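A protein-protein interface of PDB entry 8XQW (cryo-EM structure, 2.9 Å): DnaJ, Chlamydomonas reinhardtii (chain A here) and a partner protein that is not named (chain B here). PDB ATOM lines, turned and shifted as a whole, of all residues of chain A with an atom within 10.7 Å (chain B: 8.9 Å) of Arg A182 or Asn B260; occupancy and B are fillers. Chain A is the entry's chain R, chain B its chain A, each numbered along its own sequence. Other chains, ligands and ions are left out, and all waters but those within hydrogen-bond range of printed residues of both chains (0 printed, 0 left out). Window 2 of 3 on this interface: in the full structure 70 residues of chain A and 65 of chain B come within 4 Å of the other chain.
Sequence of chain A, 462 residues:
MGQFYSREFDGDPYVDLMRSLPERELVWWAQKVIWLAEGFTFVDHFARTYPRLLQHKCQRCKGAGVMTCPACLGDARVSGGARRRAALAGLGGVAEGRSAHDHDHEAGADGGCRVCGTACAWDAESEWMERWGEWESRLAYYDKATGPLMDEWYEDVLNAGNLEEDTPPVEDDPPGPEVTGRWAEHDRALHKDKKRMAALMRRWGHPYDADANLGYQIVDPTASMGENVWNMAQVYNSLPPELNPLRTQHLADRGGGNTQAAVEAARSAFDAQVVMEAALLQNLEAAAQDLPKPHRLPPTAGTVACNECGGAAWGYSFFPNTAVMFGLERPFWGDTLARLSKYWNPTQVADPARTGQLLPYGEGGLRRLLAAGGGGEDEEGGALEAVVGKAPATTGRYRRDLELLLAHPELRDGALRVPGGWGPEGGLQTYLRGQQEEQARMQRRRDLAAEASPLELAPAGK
Asn B260 touches Arg A182.
Leu A405 touches Gly B246.
Gly B246 touches Arg A412.
Asn B260 touches Arg A412.
Pro B252 touches Gly A414.
The guanidinium group of Arg A182 is in salt-bridge range of the side-chain carboxylate of Asp A413 (2.9 Å).
O of Asp A413 sits at hydrogen-bond distance from NH1 of Arg B261 (3.1 Å).
The backbone NH of Gly A414 sits at hydrogen-bond distance from the backbone carbonyl oxygen of His B259 (2.6 Å).
The side-chain carboxylate (OD1) of Asp A413 lies close to the backbone carbonyl oxygen (O) of His B259 (2.9 Å).
The guanidinium group of Arg B261 is in hydrogen-bond range of the backbone carbonyl oxygen of Leu A416 (3.1 Å).
N of Arg B261 sits at hydrogen-bond distance from O of Arg A412 (2.7 Å).
OD1 of Asn B260 lies close to OD1 of Asp A413, 3.3 Å away.
No residue of chain B comes within 4 Å of Gly A181.
Arg A182 touches just one residue of chain B: Asn B260 (3.8 Å).
Of the printed residues of chain B, Leu A405 touches Gly B246.
Printed residues of chain B within 4 Å of Gly A414: Pro B252 (3.7 Å) and His B259 (2.6 Å).
No residue of chain A comes within 4 Å of Glu B255.
No residue of chain A comes within 4 Å of Asp B256.
No residue of chain A comes within 4 Å of Ala B258.
Printed residues of chain A within 4 Å of His B259: Asp A413 and Gly A414.
Of the printed residues of chain A, Arg B261 touches Arg A412, Asp A413 and Leu A416.
No residue of chain A comes within 4 Å of Val B262.
The nearest residue of chain B that does not touch Arg A182 is Ala B258 (4.6 Å).
The nearest residue of chain A that does not touch Asn B260 is Gly A414 (4.2 Å).
The nearest printed residue of chain B that does not touch Gly A414 is Glu B255 (4.2 Å).
Of the 24 printed residues of chain A, 6 touch a printed residue of chain B.
Printed residues of chain A that touch a printed residue of chain B: Arg A182, Leu A405, Arg A412, Asp A413, Gly A414 and Leu A416.
Hydrophobic or aromatic side chains of chain A that line the printed part of chain B: Leu A405.
Of the 13 printed residues of chain B, 5 touch a printed residue of chain A.
Printed residues of chain B that touch a printed residue of chain A: Gly B246, Pro B252, His B259, Asn B260 and Arg B261.
Hydrophobic or aromatic side chains of chain B that line the printed part of chain A: Pro B252.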
ATOM      1  N   PRO A 175      15.851  22.401 -12.325  1.00  0.00           N
ATOM      2  CA  PRO A 175      15.381  21.534 -13.407  1.00  0.00           C
ATOM      3  C   PRO A 175      15.044  22.363 -14.633  1.00  0.00           C
ATOM      4  O   PRO A 175      14.593  23.505 -14.526  1.00  0.00           O
ATOM      5  CB  PRO A 175      14.132  20.868 -12.816  1.00  0.00           C
ATOM      6  CG  PRO A 175      14.252  21.048 -11.340  1.00  0.00           C
ATOM      7  CD  PRO A 175      14.969  22.341 -11.147  1.00  0.00           C
ATOM      8  N   GLU A 178       9.281  21.772 -18.552  1.00  0.00           N
ATOM      9  CA  GLU A 178       8.539  20.628 -19.074  1.00  0.00           C
ATOM     10  C   GLU A 178       8.481  19.462 -18.097  1.00  0.00           C
ATOM     11  O   GLU A 178       8.103  18.353 -18.493  1.00  0.00           O
ATOM     12  CB  GLU A 178       9.099  20.135 -20.417  1.00  0.00           C
ATOM     13  CG  GLU A 178       8.522  20.830 -21.642  1.00  0.00           C
ATOM     14  CD  GLU A 178       8.595  22.341 -21.552  1.00  0.00           C
ATOM     15  OE1 GLU A 178       9.701  22.870 -21.323  1.00  0.00           O
ATOM     16  OE2 GLU A 178       7.547  23.002 -21.709  1.00  0.00           O
ATOM     17  N   VAL A 179       8.852  19.667 -16.837  1.00  0.00           N
ATOM     18  CA  VAL A 179       8.648  18.666 -15.798  1.00  0.00           C
ATOM     19  C   VAL A 179       7.649  19.232 -14.792  1.00  0.00           C
ATOM     20  O   VAL A 179       7.998  20.050 -13.937  1.00  0.00           O
ATOM     21  CB  VAL A 179       9.969  18.255 -15.135  1.00  0.00           C
ATOM     22  CG1 VAL A 179      10.817  19.468 -14.780  1.00  0.00           C
ATOM     23  CG2 VAL A 179       9.704  17.397 -13.906  1.00  0.00           C
ATOM     24  N   THR A 180       6.391  18.810 -14.907  1.00  0.00           N
ATOM     25  CA  THR A 180       5.322  19.349 -14.074  1.00  0.00           C
ATOM     26  C   THR A 180       5.309  18.619 -12.737  1.00  0.00           C
ATOM     27  O   THR A 180       5.432  17.391 -12.685  1.00  0.00           O
ATOM     28  CB  THR A 180       3.976  19.232 -14.784  1.00  0.00           C
ATOM     29  OG1 THR A 180       2.919  19.449 -13.841  1.00  0.00           O
ATOM     30  CG2 THR A 180       3.819  17.860 -15.418  1.00  0.00           C
ATOM     31  N   GLY A 181       5.170  19.376 -11.656  1.00  0.00           N
ATOM     32  CA  GLY A 181       5.214  18.806 -10.324  1.00  0.00           C
ATOM     33  C   GLY A 181       5.421  19.909  -9.311  1.00  0.00           C
ATOM     34  O   GLY A 181       5.611  21.078  -9.659  1.00  0.00           O
ATOM     35  N   ARG A 182       5.391  19.512  -8.039  1.00  0.00           N
ATOM     36  CA  ARG A 182       5.514  20.488  -6.961  1.00  0.00           C
ATOM     37  C   ARG A 182       6.972  20.778  -6.630  1.00  0.00           C
ATOM     38  O   ARG A 182       7.368  21.945  -6.510  1.00  0.00           O
ATOM     39  CB  ARG A 182       4.770  19.982  -5.727  1.00  0.00           C
ATOM     40  CG  ARG A 182       4.832  20.906  -4.533  1.00  0.00           C
ATOM     41  CD  ARG A 182       3.969  20.381  -3.403  1.00  0.00           C
ATOM     42  NE  ARG A 182       2.547  20.491  -3.720  1.00  0.00           N
ATOM     43  CZ  ARG A 182       1.748  21.449  -3.261  1.00  0.00           C
ATOM     44  NH1 ARG A 182       2.227  22.387  -2.456  1.00  0.00           N
ATOM     45  NH2 ARG A 182       0.469  21.468  -3.608  1.00  0.00           N
ATOM     46  N   TRP A 183       7.776  19.728  -6.470  1.00  0.00           N
ATOM     47  CA  TRP A 183       9.196  19.908  -6.197  1.00  0.00           C
ATOM     48  C   TRP A 183       9.862  20.741  -7.283  1.00  0.00           C
ATOM     49  O   TRP A 183      10.720  21.590  -6.998  1.00  0.00           O
ATOM     50  CB  TRP A 183       9.855  18.539  -6.079  1.00  0.00           C
ATOM     51  CG  TRP A 183      11.226  18.574  -5.546  1.00  0.00           C
ATOM     52  CD1 TRP A 183      11.598  18.491  -4.241  1.00  0.00           C
ATOM     53  CD2 TRP A 183      12.432  18.687  -6.303  1.00  0.00           C
ATOM     54  NE1 TRP A 183      12.965  18.551  -4.135  1.00  0.00           N
ATOM     55  CE2 TRP A 183      13.500  18.670  -5.389  1.00  0.00           C
ATOM     56  CE3 TRP A 183      12.711  18.805  -7.667  1.00  0.00           C
ATOM     57  CZ2 TRP A 183      14.826  18.765  -5.792  1.00  0.00           C
ATOM     58  CZ3 TRP A 183      14.024  18.899  -8.066  1.00  0.00           C
ATOM     59  CH2 TRP A 183      15.068  18.874  -7.133  1.00  0.00           C
ATOM     60  N   ALA A 184       9.473  20.512  -8.538  1.00  0.00           N
ATOM     61  CA  ALA A 184      10.004  21.304  -9.639  1.00  0.00           C
ATOM     62  C   ALA A 184       9.664  22.776  -9.473  1.00  0.00           C
ATOM     63  O   ALA A 184      10.516  23.639  -9.695  1.00  0.00           O
ATOM     64  CB  ALA A 184       9.467  20.776 -10.967  1.00  0.00           C
ATOM     65  N   GLU A 185       8.426  23.084  -9.086  1.00  0.00           N
ATOM     66  CA  GLU A 185       8.038  24.477  -8.887  1.00  0.00           C
ATOM     67  C   GLU A 185       8.843  25.112  -7.765  1.00  0.00           C
ATOM     68  O   GLU A 185       9.313  26.249  -7.887  1.00  0.00           O
ATOM     69  CB  GLU A 185       6.545  24.567  -8.590  1.00  0.00           C
ATOM     70  CG  GLU A 185       5.669  24.233  -9.771  1.00  0.00           C
ATOM     71  CD  GLU A 185       4.273  23.850  -9.358  1.00  0.00           C
ATOM     72  OE1 GLU A 185       3.656  23.013 -10.050  1.00  0.00           O
ATOM     73  OE2 GLU A 185       3.791  24.380  -8.337  1.00  0.00           O
ATOM     74  N   HIS A 186       8.997  24.391  -6.652  1.00  0.00           N
ATOM     75  CA  HIS A 186       9.801  24.903  -5.549  1.00  0.00           C
ATOM     76  C   HIS A 186      11.199  25.265  -6.022  1.00  0.00           C
ATOM     77  O   HIS A 186      11.661  26.395  -5.825  1.00  0.00           O
ATOM     78  CB  HIS A 186       9.879  23.874  -4.422  1.00  0.00           C
ATOM     79  CG  HIS A 186       8.569  23.583  -3.769  1.00  0.00           C
ATOM     80  ND1 HIS A 186       8.393  22.523  -2.907  1.00  0.00           N
ATOM     81  CD2 HIS A 186       7.374  24.209  -3.849  1.00  0.00           C
ATOM     82  CE1 HIS A 186       7.141  22.509  -2.485  1.00  0.00           C
ATOM     83  NE2 HIS A 186       6.501  23.520  -3.043  1.00  0.00           N
ATOM     84  N   ASP A 187      11.882  24.317  -6.668  1.00  0.00           N
ATOM     85  CA  ASP A 187      13.256  24.568  -7.090  1.00  0.00           C
ATOM     86  C   ASP A 187      13.333  25.687  -8.120  1.00  0.00           C
ATOM     87  O   ASP A 187      14.228  26.539  -8.053  1.00  0.00           O
ATOM     88  CB  ASP A 187      13.883  23.291  -7.636  1.00  0.00           C
ATOM     89  CG  ASP A 187      14.982  22.765  -6.744  1.00  0.00           C
ATOM     90  OD1 ASP A 187      15.232  23.376  -5.688  1.00  0.00           O
ATOM     91  OD2 ASP A 187      15.613  21.754  -7.104  1.00  0.00           O
ATOM     92  N   ARG A 188      12.400  25.715  -9.074  1.00  0.00           N
ATOM     93  CA  ARG A 188      12.449  26.729 -10.116  1.00  0.00           C
ATOM     94  C   ARG A 188      12.269  28.122  -9.537  1.00  0.00           C
ATOM     95  O   ARG A 188      13.020  29.042  -9.876  1.00  0.00           O
ATOM     96  CB  ARG A 188      11.383  26.450 -11.171  1.00  0.00           C
ATOM     97  CG  ARG A 188      11.712  25.296 -12.093  1.00  0.00           C
ATOM     98  CD  ARG A 188      10.902  25.375 -13.372  1.00  0.00           C
ATOM     99  NE  ARG A 188       9.545  24.868 -13.188  1.00  0.00           N
ATOM    100  CZ  ARG A 188       8.491  25.637 -12.944  1.00  0.00           C
ATOM    101  NH1 ARG A 188       8.632  26.951 -12.859  1.00  0.00           N
ATOM    102  NH2 ARG A 188       7.292  25.093 -12.790  1.00  0.00           N
ATOM    103  N   ALA A 189      11.285  28.300  -8.656  1.00  0.00           N
ATOM    104  CA  ALA A 189      11.096  29.613  -8.053  1.00  0.00           C
ATOM    105  C   ALA A 189      12.253  29.959  -7.127  1.00  0.00           C
ATOM    106  O   ALA A 189      12.575  31.138  -6.942  1.00  0.00           O
ATOM    107  CB  ALA A 189       9.766  29.669  -7.307  1.00  0.00           C
ATOM    108  N   LEU A 190      12.895  28.950  -6.538  1.00  0.00           N
ATOM    109  CA  LEU A 190      13.992  29.232  -5.624  1.00  0.00           C
ATOM    110  C   LEU A 190      15.240  29.688  -6.367  1.00  0.00           C
ATOM    111  O   LEU A 190      15.971  30.553  -5.875  1.00  0.00           O
ATOM    112  CB  LEU A 190      14.283  27.995  -4.775  1.00  0.00           C
ATOM    113  CG  LEU A 190      15.422  28.034  -3.756  1.00  0.00           C
ATOM    114  CD1 LEU A 190      15.025  27.220  -2.543  1.00  0.00           C
ATOM    115  CD2 LEU A 190      16.710  27.496  -4.346  1.00  0.00           C
ATOM    116  N   LEU A 405     -12.725  28.603   2.189  1.00  0.00           N
ATOM    117  CA  LEU A 405     -11.624  27.741   2.589  1.00  0.00           C
ATOM    118  C   LEU A 405     -11.951  26.270   2.404  1.00  0.00           C
ATOM    119  O   LEU A 405     -11.064  25.424   2.556  1.00  0.00           O
ATOM    120  CB  LEU A 405     -11.253  28.013   4.040  1.00  0.00           C
ATOM    121  CG  LEU A 405      -9.807  27.723   4.409  1.00  0.00           C
ATOM    122  CD1 LEU A 405      -8.889  28.312   3.368  1.00  0.00           C
ATOM    123  CD2 LEU A 405      -9.509  28.298   5.769  1.00  0.00           C
ATOM    124  N   HIS A 408     -11.671  25.661  -2.038  1.00  0.00           N
ATOM    125  CA  HIS A 408     -10.369  25.843  -2.672  1.00  0.00           C
ATOM    126  C   HIS A 408      -9.299  25.318  -1.730  1.00  0.00           C
ATOM    127  O   HIS A 408      -8.602  26.098  -1.071  1.00  0.00           O
ATOM    128  CB  HIS A 408     -10.126  27.311  -3.010  1.00  0.00           C
ATOM    129  CG  HIS A 408     -11.256  27.957  -3.746  1.00  0.00           C
ATOM    130  ND1 HIS A 408     -12.433  28.318  -3.131  1.00  0.00           N
ATOM    131  CD2 HIS A 408     -11.385  28.316  -5.043  1.00  0.00           C
ATOM    132  CE1 HIS A 408     -13.242  28.866  -4.019  1.00  0.00           C
ATOM    133  NE2 HIS A 408     -12.629  28.879  -5.187  1.00  0.00           N
ATOM    134  N   PRO A 409      -9.138  23.998  -1.644  1.00  0.00           N
ATOM    135  CA  PRO A 409      -8.147  23.444  -0.708  1.00  0.00           C
ATOM    136  C   PRO A 409      -6.738  23.933  -0.961  1.00  0.00           C
ATOM    137  O   PRO A 409      -5.959  24.075  -0.011  1.00  0.00           O
ATOM    138  CB  PRO A 409      -8.267  21.932  -0.928  1.00  0.00           C
ATOM    139  CG  PRO A 409      -9.626  21.739  -1.494  1.00  0.00           C
ATOM    140  CD  PRO A 409      -9.889  22.942  -2.339  1.00  0.00           C
ATOM    141  N   GLU A 410      -6.390  24.218  -2.216  1.00  0.00           N
ATOM    142  CA  GLU A 410      -5.039  24.654  -2.548  1.00  0.00           C
ATOM    143  C   GLU A 410      -4.607  25.897  -1.785  1.00  0.00           C
ATOM    144  O   GLU A 410      -3.405  26.178  -1.729  1.00  0.00           O
ATOM    145  CB  GLU A 410      -4.932  24.921  -4.046  1.00  0.00           C
ATOM    146  CG  GLU A 410      -5.578  26.222  -4.489  1.00  0.00           C
ATOM    147  CD  GLU A 410      -7.068  26.084  -4.725  1.00  0.00           C
ATOM    148  OE1 GLU A 410      -7.619  24.992  -4.473  1.00  0.00           O
ATOM    149  OE2 GLU A 410      -7.689  27.070  -5.171  1.00  0.00           O
ATOM    150  N   LEU A 411      -5.543  26.642  -1.195  1.00  0.00           N
ATOM    151  CA  LEU A 411      -5.178  27.822  -0.429  1.00  0.00           C
ATOM    152  C   LEU A 411      -4.456  27.485   0.864  1.00  0.00           C
ATOM    153  O   LEU A 411      -3.902  28.391   1.492  1.00  0.00           O
ATOM    154  CB  LEU A 411      -6.420  28.651  -0.113  1.00  0.00           C
ATOM    155  CG  LEU A 411      -7.162  29.203  -1.326  1.00  0.00           C
ATOM    156  CD1 LEU A 411      -8.503  29.762  -0.910  1.00  0.00           C
ATOM    157  CD2 LEU A 411      -6.334  30.269  -2.007  1.00  0.00           C
ATOM    158  N   ARG A 412      -4.441  26.221   1.276  1.00  0.00           N
ATOM    159  CA  ARG A 412      -3.766  25.821   2.502  1.00  0.00           C
ATOM    160  C   ARG A 412      -2.301  25.480   2.280  1.00  0.00           C
ATOM    161  O   ARG A 412      -1.713  24.757   3.091  1.00  0.00           O
ATOM    162  CB  ARG A 412      -4.489  24.635   3.136  1.00  0.00           C
ATOM    163  CG  ARG A 412      -5.990  24.784   3.160  1.00  0.00           C
ATOM    164  CD  ARG A 412      -6.580  24.054   4.335  1.00  0.00           C
ATOM    165  NE  ARG A 412      -5.894  22.791   4.550  1.00  0.00           N
ATOM    166  CZ  ARG A 412      -6.258  21.649   3.989  1.00  0.00           C
ATOM    167  NH1 ARG A 412      -7.304  21.616   3.178  1.00  0.00           N
ATOM    168  NH2 ARG A 412      -5.579  20.541   4.240  1.00  0.00           N
ATOM    169  N   ASP A 413      -1.699  25.987   1.210  1.00  0.00           N
ATOM    170  CA  ASP A 413      -0.330  25.624   0.880  1.00  0.00           C
ATOM    171  C   ASP A 413       0.650  26.362   1.781  1.00  0.00           C
ATOM    172  O   ASP A 413       0.474  27.543   2.084  1.00  0.00           O
ATOM    173  CB  ASP A 413      -0.041  25.938  -0.583  1.00  0.00           C
ATOM    174  CG  ASP A 413       1.177  25.208  -1.101  1.00  0.00           C
ATOM    175  OD1 ASP A 413       1.917  24.632  -0.280  1.00  0.00           O
ATOM    176  OD2 ASP A 413       1.387  25.203  -2.331  1.00  0.00           O
ATOM    177  N   GLY A 414       1.704  25.655   2.195  1.00  0.00           N
ATOM    178  CA  GLY A 414       2.654  26.212   3.138  1.00  0.00           C
ATOM    179  C   GLY A 414       3.464  27.370   2.600  1.00  0.00           C
ATOM    180  O   GLY A 414       4.195  28.006   3.365  1.00  0.00           O
ATOM    181  N   ALA A 415       3.361  27.658   1.305  1.00  0.00           N
ATOM    182  CA  ALA A 415       4.164  28.716   0.713  1.00  0.00           C
ATOM    183  C   ALA A 415       3.484  30.075   0.761  1.00  0.00           C
ATOM    184  O   ALA A 415       4.167  31.096   0.657  1.00  0.00           O
ATOM    185  CB  ALA A 415       4.500  28.368  -0.735  1.00  0.00           C
ATOM    186  N   LEU A 416       2.170  30.109   0.924  1.00  0.00           N
ATOM    187  CA  LEU A 416       1.391  31.333   0.835  1.00  0.00           C
ATOM    188  C   LEU A 416       1.134  31.905   2.224  1.00  0.00           C
ATOM    189  O   LEU A 416       1.000  31.158   3.197  1.00  0.00           O
ATOM    190  CB  LEU A 416       0.073  31.051   0.120  1.00  0.00           C
ATOM    191  CG  LEU A 416      -1.010  32.118   0.143  1.00  0.00           C
ATOM    192  CD1 LEU A 416      -0.518  33.374  -0.541  1.00  0.00           C
ATOM    193  CD2 LEU A 416      -2.263  31.591  -0.524  1.00  0.00           C
ATOM    194  N   GLY B 246      -6.973  25.492   8.412  1.00  0.00           N
ATOM    195  CA  GLY B 246      -5.811  25.783   7.610  1.00  0.00           C
ATOM    196  C   GLY B 246      -5.925  27.119   6.914  1.00  0.00           C
ATOM    197  O   GLY B 246      -5.772  27.193   5.695  1.00  0.00           O
ATOM    198  N   PRO B 252       2.740  28.890   9.154  1.00  0.00           N
ATOM    199  CA  PRO B 252       2.585  27.447   8.882  1.00  0.00           C
ATOM    200  C   PRO B 252       3.259  26.576   9.938  1.00  0.00           C
ATOM    201  O   PRO B 252       4.359  26.061   9.776  1.00  0.00           O
ATOM    202  CB  PRO B 252       3.245  27.292   7.511  1.00  0.00           C
ATOM    203  CG  PRO B 252       3.287  28.665   6.940  1.00  0.00           C
ATOM    204  CD  PRO B 252       3.511  29.558   8.100  1.00  0.00           C
ATOM    205  N   PHE B 253       2.568  26.407  11.065  1.00  0.00           N
ATOM    206  CA  PHE B 253       3.135  25.637  12.167  1.00  0.00           C
ATOM    207  C   PHE B 253       3.155  24.149  11.845  1.00  0.00           C
ATOM    208  O   PHE B 253       4.166  23.471  12.057  1.00  0.00           O
ATOM    209  CB  PHE B 253       2.338  25.884  13.445  1.00  0.00           C
ATOM    210  CG  PHE B 253       2.691  27.151  14.160  1.00  0.00           C
ATOM    211  CD1 PHE B 253       3.783  27.204  14.999  1.00  0.00           C
ATOM    212  CD2 PHE B 253       1.910  28.276  14.023  1.00  0.00           C
ATOM    213  CE1 PHE B 253       4.101  28.360  15.665  1.00  0.00           C
ATOM    214  CE2 PHE B 253       2.224  29.432  14.691  1.00  0.00           C
ATOM    215  CZ  PHE B 253       3.321  29.475  15.508  1.00  0.00           C
ATOM    216  N   TYR B 254       2.042  23.621  11.344  1.00  0.00           N
ATOM    217  CA  TYR B 254       1.841  22.187  11.187  1.00  0.00           C
ATOM    218  C   TYR B 254       1.531  21.873   9.735  1.00  0.00           C
ATOM    219  O   TYR B 254       0.529  22.351   9.195  1.00  0.00           O
ATOM    220  CB  TYR B 254       0.708  21.701  12.088  1.00  0.00           C
ATOM    221  CG  TYR B 254       0.625  22.454  13.391  1.00  0.00           C
ATOM    222  CD1 TYR B 254       1.484  22.161  14.435  1.00  0.00           C
ATOM    223  CD2 TYR B 254      -0.298  23.468  13.571  1.00  0.00           C
ATOM    224  CE1 TYR B 254       1.421  22.848  15.615  1.00  0.00           C
ATOM    225  CE2 TYR B 254      -0.368  24.158  14.754  1.00  0.00           C
ATOM    226  CZ  TYR B 254       0.496  23.845  15.771  1.00  0.00           C
ATOM    227  OH  TYR B 254       0.436  24.530  16.957  1.00  0.00           O
ATOM    228  N   GLU B 255       2.375  21.053   9.112  1.00  0.00           N
ATOM    229  CA  GLU B 255       2.312  20.816   7.680  1.00  0.00           C
ATOM    230  C   GLU B 255       2.252  19.328   7.376  1.00  0.00           C
ATOM    231  O   GLU B 255       2.777  18.492   8.113  1.00  0.00           O
ATOM    232  CB  GLU B 255       3.519  21.429   6.963  1.00  0.00           C
ATOM    233  CG  GLU B 255       3.445  22.929   6.784  1.00  0.00           C
ATOM    234  CD  GLU B 255       4.805  23.585   6.874  1.00  0.00           C
ATOM    235  OE1 GLU B 255       5.575  23.230   7.789  1.00  0.00           O
ATOM    236  OE2 GLU B 255       5.110  24.448   6.026  1.00  0.00           O
ATOM    237  N   ASP B 256       1.613  19.022   6.253  1.00  0.00           N
ATOM    238  CA  ASP B 256       1.561  17.691   5.673  1.00  0.00           C
ATOM    239  C   ASP B 256       2.914  17.387   5.030  1.00  0.00           C
ATOM    240  O   ASP B 256       3.815  18.227   5.028  1.00  0.00           O
ATOM    241  CB  ASP B 256       0.396  17.633   4.685  1.00  0.00           C
ATOM    242  CG  ASP B 256       0.256  16.292   4.004  1.00  0.00           C
ATOM    243  OD1 ASP B 256       0.807  15.304   4.521  1.00  0.00           O
ATOM    244  OD2 ASP B 256      -0.396  16.229   2.941  1.00  0.00           O
ATOM    245  N   SER B 257       3.082  16.183   4.480  1.00  0.00           N
ATOM    246  CA  SER B 257       4.290  15.884   3.716  1.00  0.00           C
ATOM    247  C   SER B 257       4.385  16.792   2.498  1.00  0.00           C
ATOM    248  O   SER B 257       5.334  17.573   2.360  1.00  0.00           O
ATOM    249  CB  SER B 257       4.294  14.415   3.306  1.00  0.00           C
ATOM    250  OG  SER B 257       2.975  13.975   3.054  1.00  0.00           O
ATOM    251  N   ALA B 258       3.405  16.711   1.607  1.00  0.00           N
ATOM    252  CA  ALA B 258       3.150  17.824   0.709  1.00  0.00           C
ATOM    253  C   ALA B 258       2.803  19.036   1.555  1.00  0.00           C
ATOM    254  O   ALA B 258       1.817  19.019   2.296  1.00  0.00           O
ATOM    255  CB  ALA B 258       2.014  17.492  -0.254  1.00  0.00           C
ATOM    256  N   HIS B 259       3.598  20.094   1.445  1.00  0.00           N
ATOM    257  CA  HIS B 259       3.619  21.096   2.501  1.00  0.00           C
ATOM    258  C   HIS B 259       2.332  21.914   2.534  1.00  0.00           C
ATOM    259  O   HIS B 259       2.324  23.097   2.181  1.00  0.00           O
ATOM    260  CB  HIS B 259       4.832  22.015   2.333  1.00  0.00           C
ATOM    261  CG  HIS B 259       6.137  21.291   2.190  1.00  0.00           C
ATOM    262  ND1 HIS B 259       7.289  21.706   2.825  1.00  0.00           N
ATOM    263  CD2 HIS B 259       6.485  20.200   1.468  1.00  0.00           C
ATOM    264  CE1 HIS B 259       8.284  20.899   2.508  1.00  0.00           C
ATOM    265  NE2 HIS B 259       7.822  19.974   1.687  1.00  0.00           N
ATOM    266  N   ASN B 260       1.239  21.289   2.968  1.00  0.00           N
ATOM    267  CA  ASN B 260      -0.043  21.954   3.151  1.00  0.00           C
ATOM    268  C   ASN B 260      -0.403  21.996   4.629  1.00  0.00           C
ATOM    269  O   ASN B 260      -0.194  21.020   5.355  1.00  0.00           O
ATOM    270  CB  ASN B 260      -1.154  21.239   2.383  1.00  0.00           C
ATOM    271  CG  ASN B 260      -1.083  21.489   0.902  1.00  0.00           C
ATOM    272  OD1 ASN B 260      -0.246  22.256   0.437  1.00  0.00           O
ATOM    273  ND2 ASN B 260      -1.968  20.849   0.149  1.00  0.00           N
ATOM    274  N   ARG B 261      -0.942  23.129   5.069  1.00  0.00           N
ATOM    275  CA  ARG B 261      -1.414  23.240   6.439  1.00  0.00           C
ATOM    276  C   ARG B 261      -2.492  22.199   6.701  1.00  0.00           C
ATOM    277  O   ARG B 261      -3.324  21.912   5.838  1.00  0.00           O
ATOM    278  CB  ARG B 261      -1.976  24.633   6.696  1.00  0.00           C
ATOM    279  CG  ARG B 261      -1.013  25.770   6.457  1.00  0.00           C
ATOM    280  CD  ARG B 261      -1.782  27.067   6.383  1.00  0.00           C
ATOM    281  NE  ARG B 261      -0.972  28.219   6.739  1.00  0.00           N
ATOM    282  CZ  ARG B 261      -0.469  29.069   5.857  1.00  0.00           C
ATOM    283  NH1 ARG B 261      -0.689  28.889   4.568  1.00  0.00           N
ATOM    284  NH2 ARG B 261       0.256  30.098   6.265  1.00  0.00           N
ATOM    285  N   VAL B 262      -2.480  21.630   7.900  1.00  0.00           N
ATOM    286  CA  VAL B 262      -3.481  20.636   8.247  1.00  0.00           C
ATOM    287  C   VAL B 262      -4.739  21.324   8.759  1.00  0.00           C
ATOM    288  O   VAL B 262      -4.712  22.453   9.248  1.00  0.00           O
ATOM    289  CB  VAL B 262      -2.941  19.638   9.278  1.00  0.00           C
ATOM    290  CG1 VAL B 262      -2.177  18.541   8.581  1.00  0.00           C
ATOM    291  CG2 VAL B 262      -2.057  20.349  10.261  1.00  0.00           C
ATOM    292  N   SER B 263      -5.859  20.623   8.633  1.00  0.00           N
ATOM    293  CA  SER B 263      -7.140  21.074   9.142  1.00  0.00           C
ATOM    294  C   SER B 263      -7.765  19.949   9.951  1.00  0.00           C
ATOM    295  O   SER B 263      -7.385  18.787   9.813  1.00  0.00           O
ATOM    296  CB  SER B 263      -8.081  21.486   8.017  1.00  0.00           C
ATOM    297  OG  SER B 263      -9.417  21.188   8.363  1.00  0.00           O
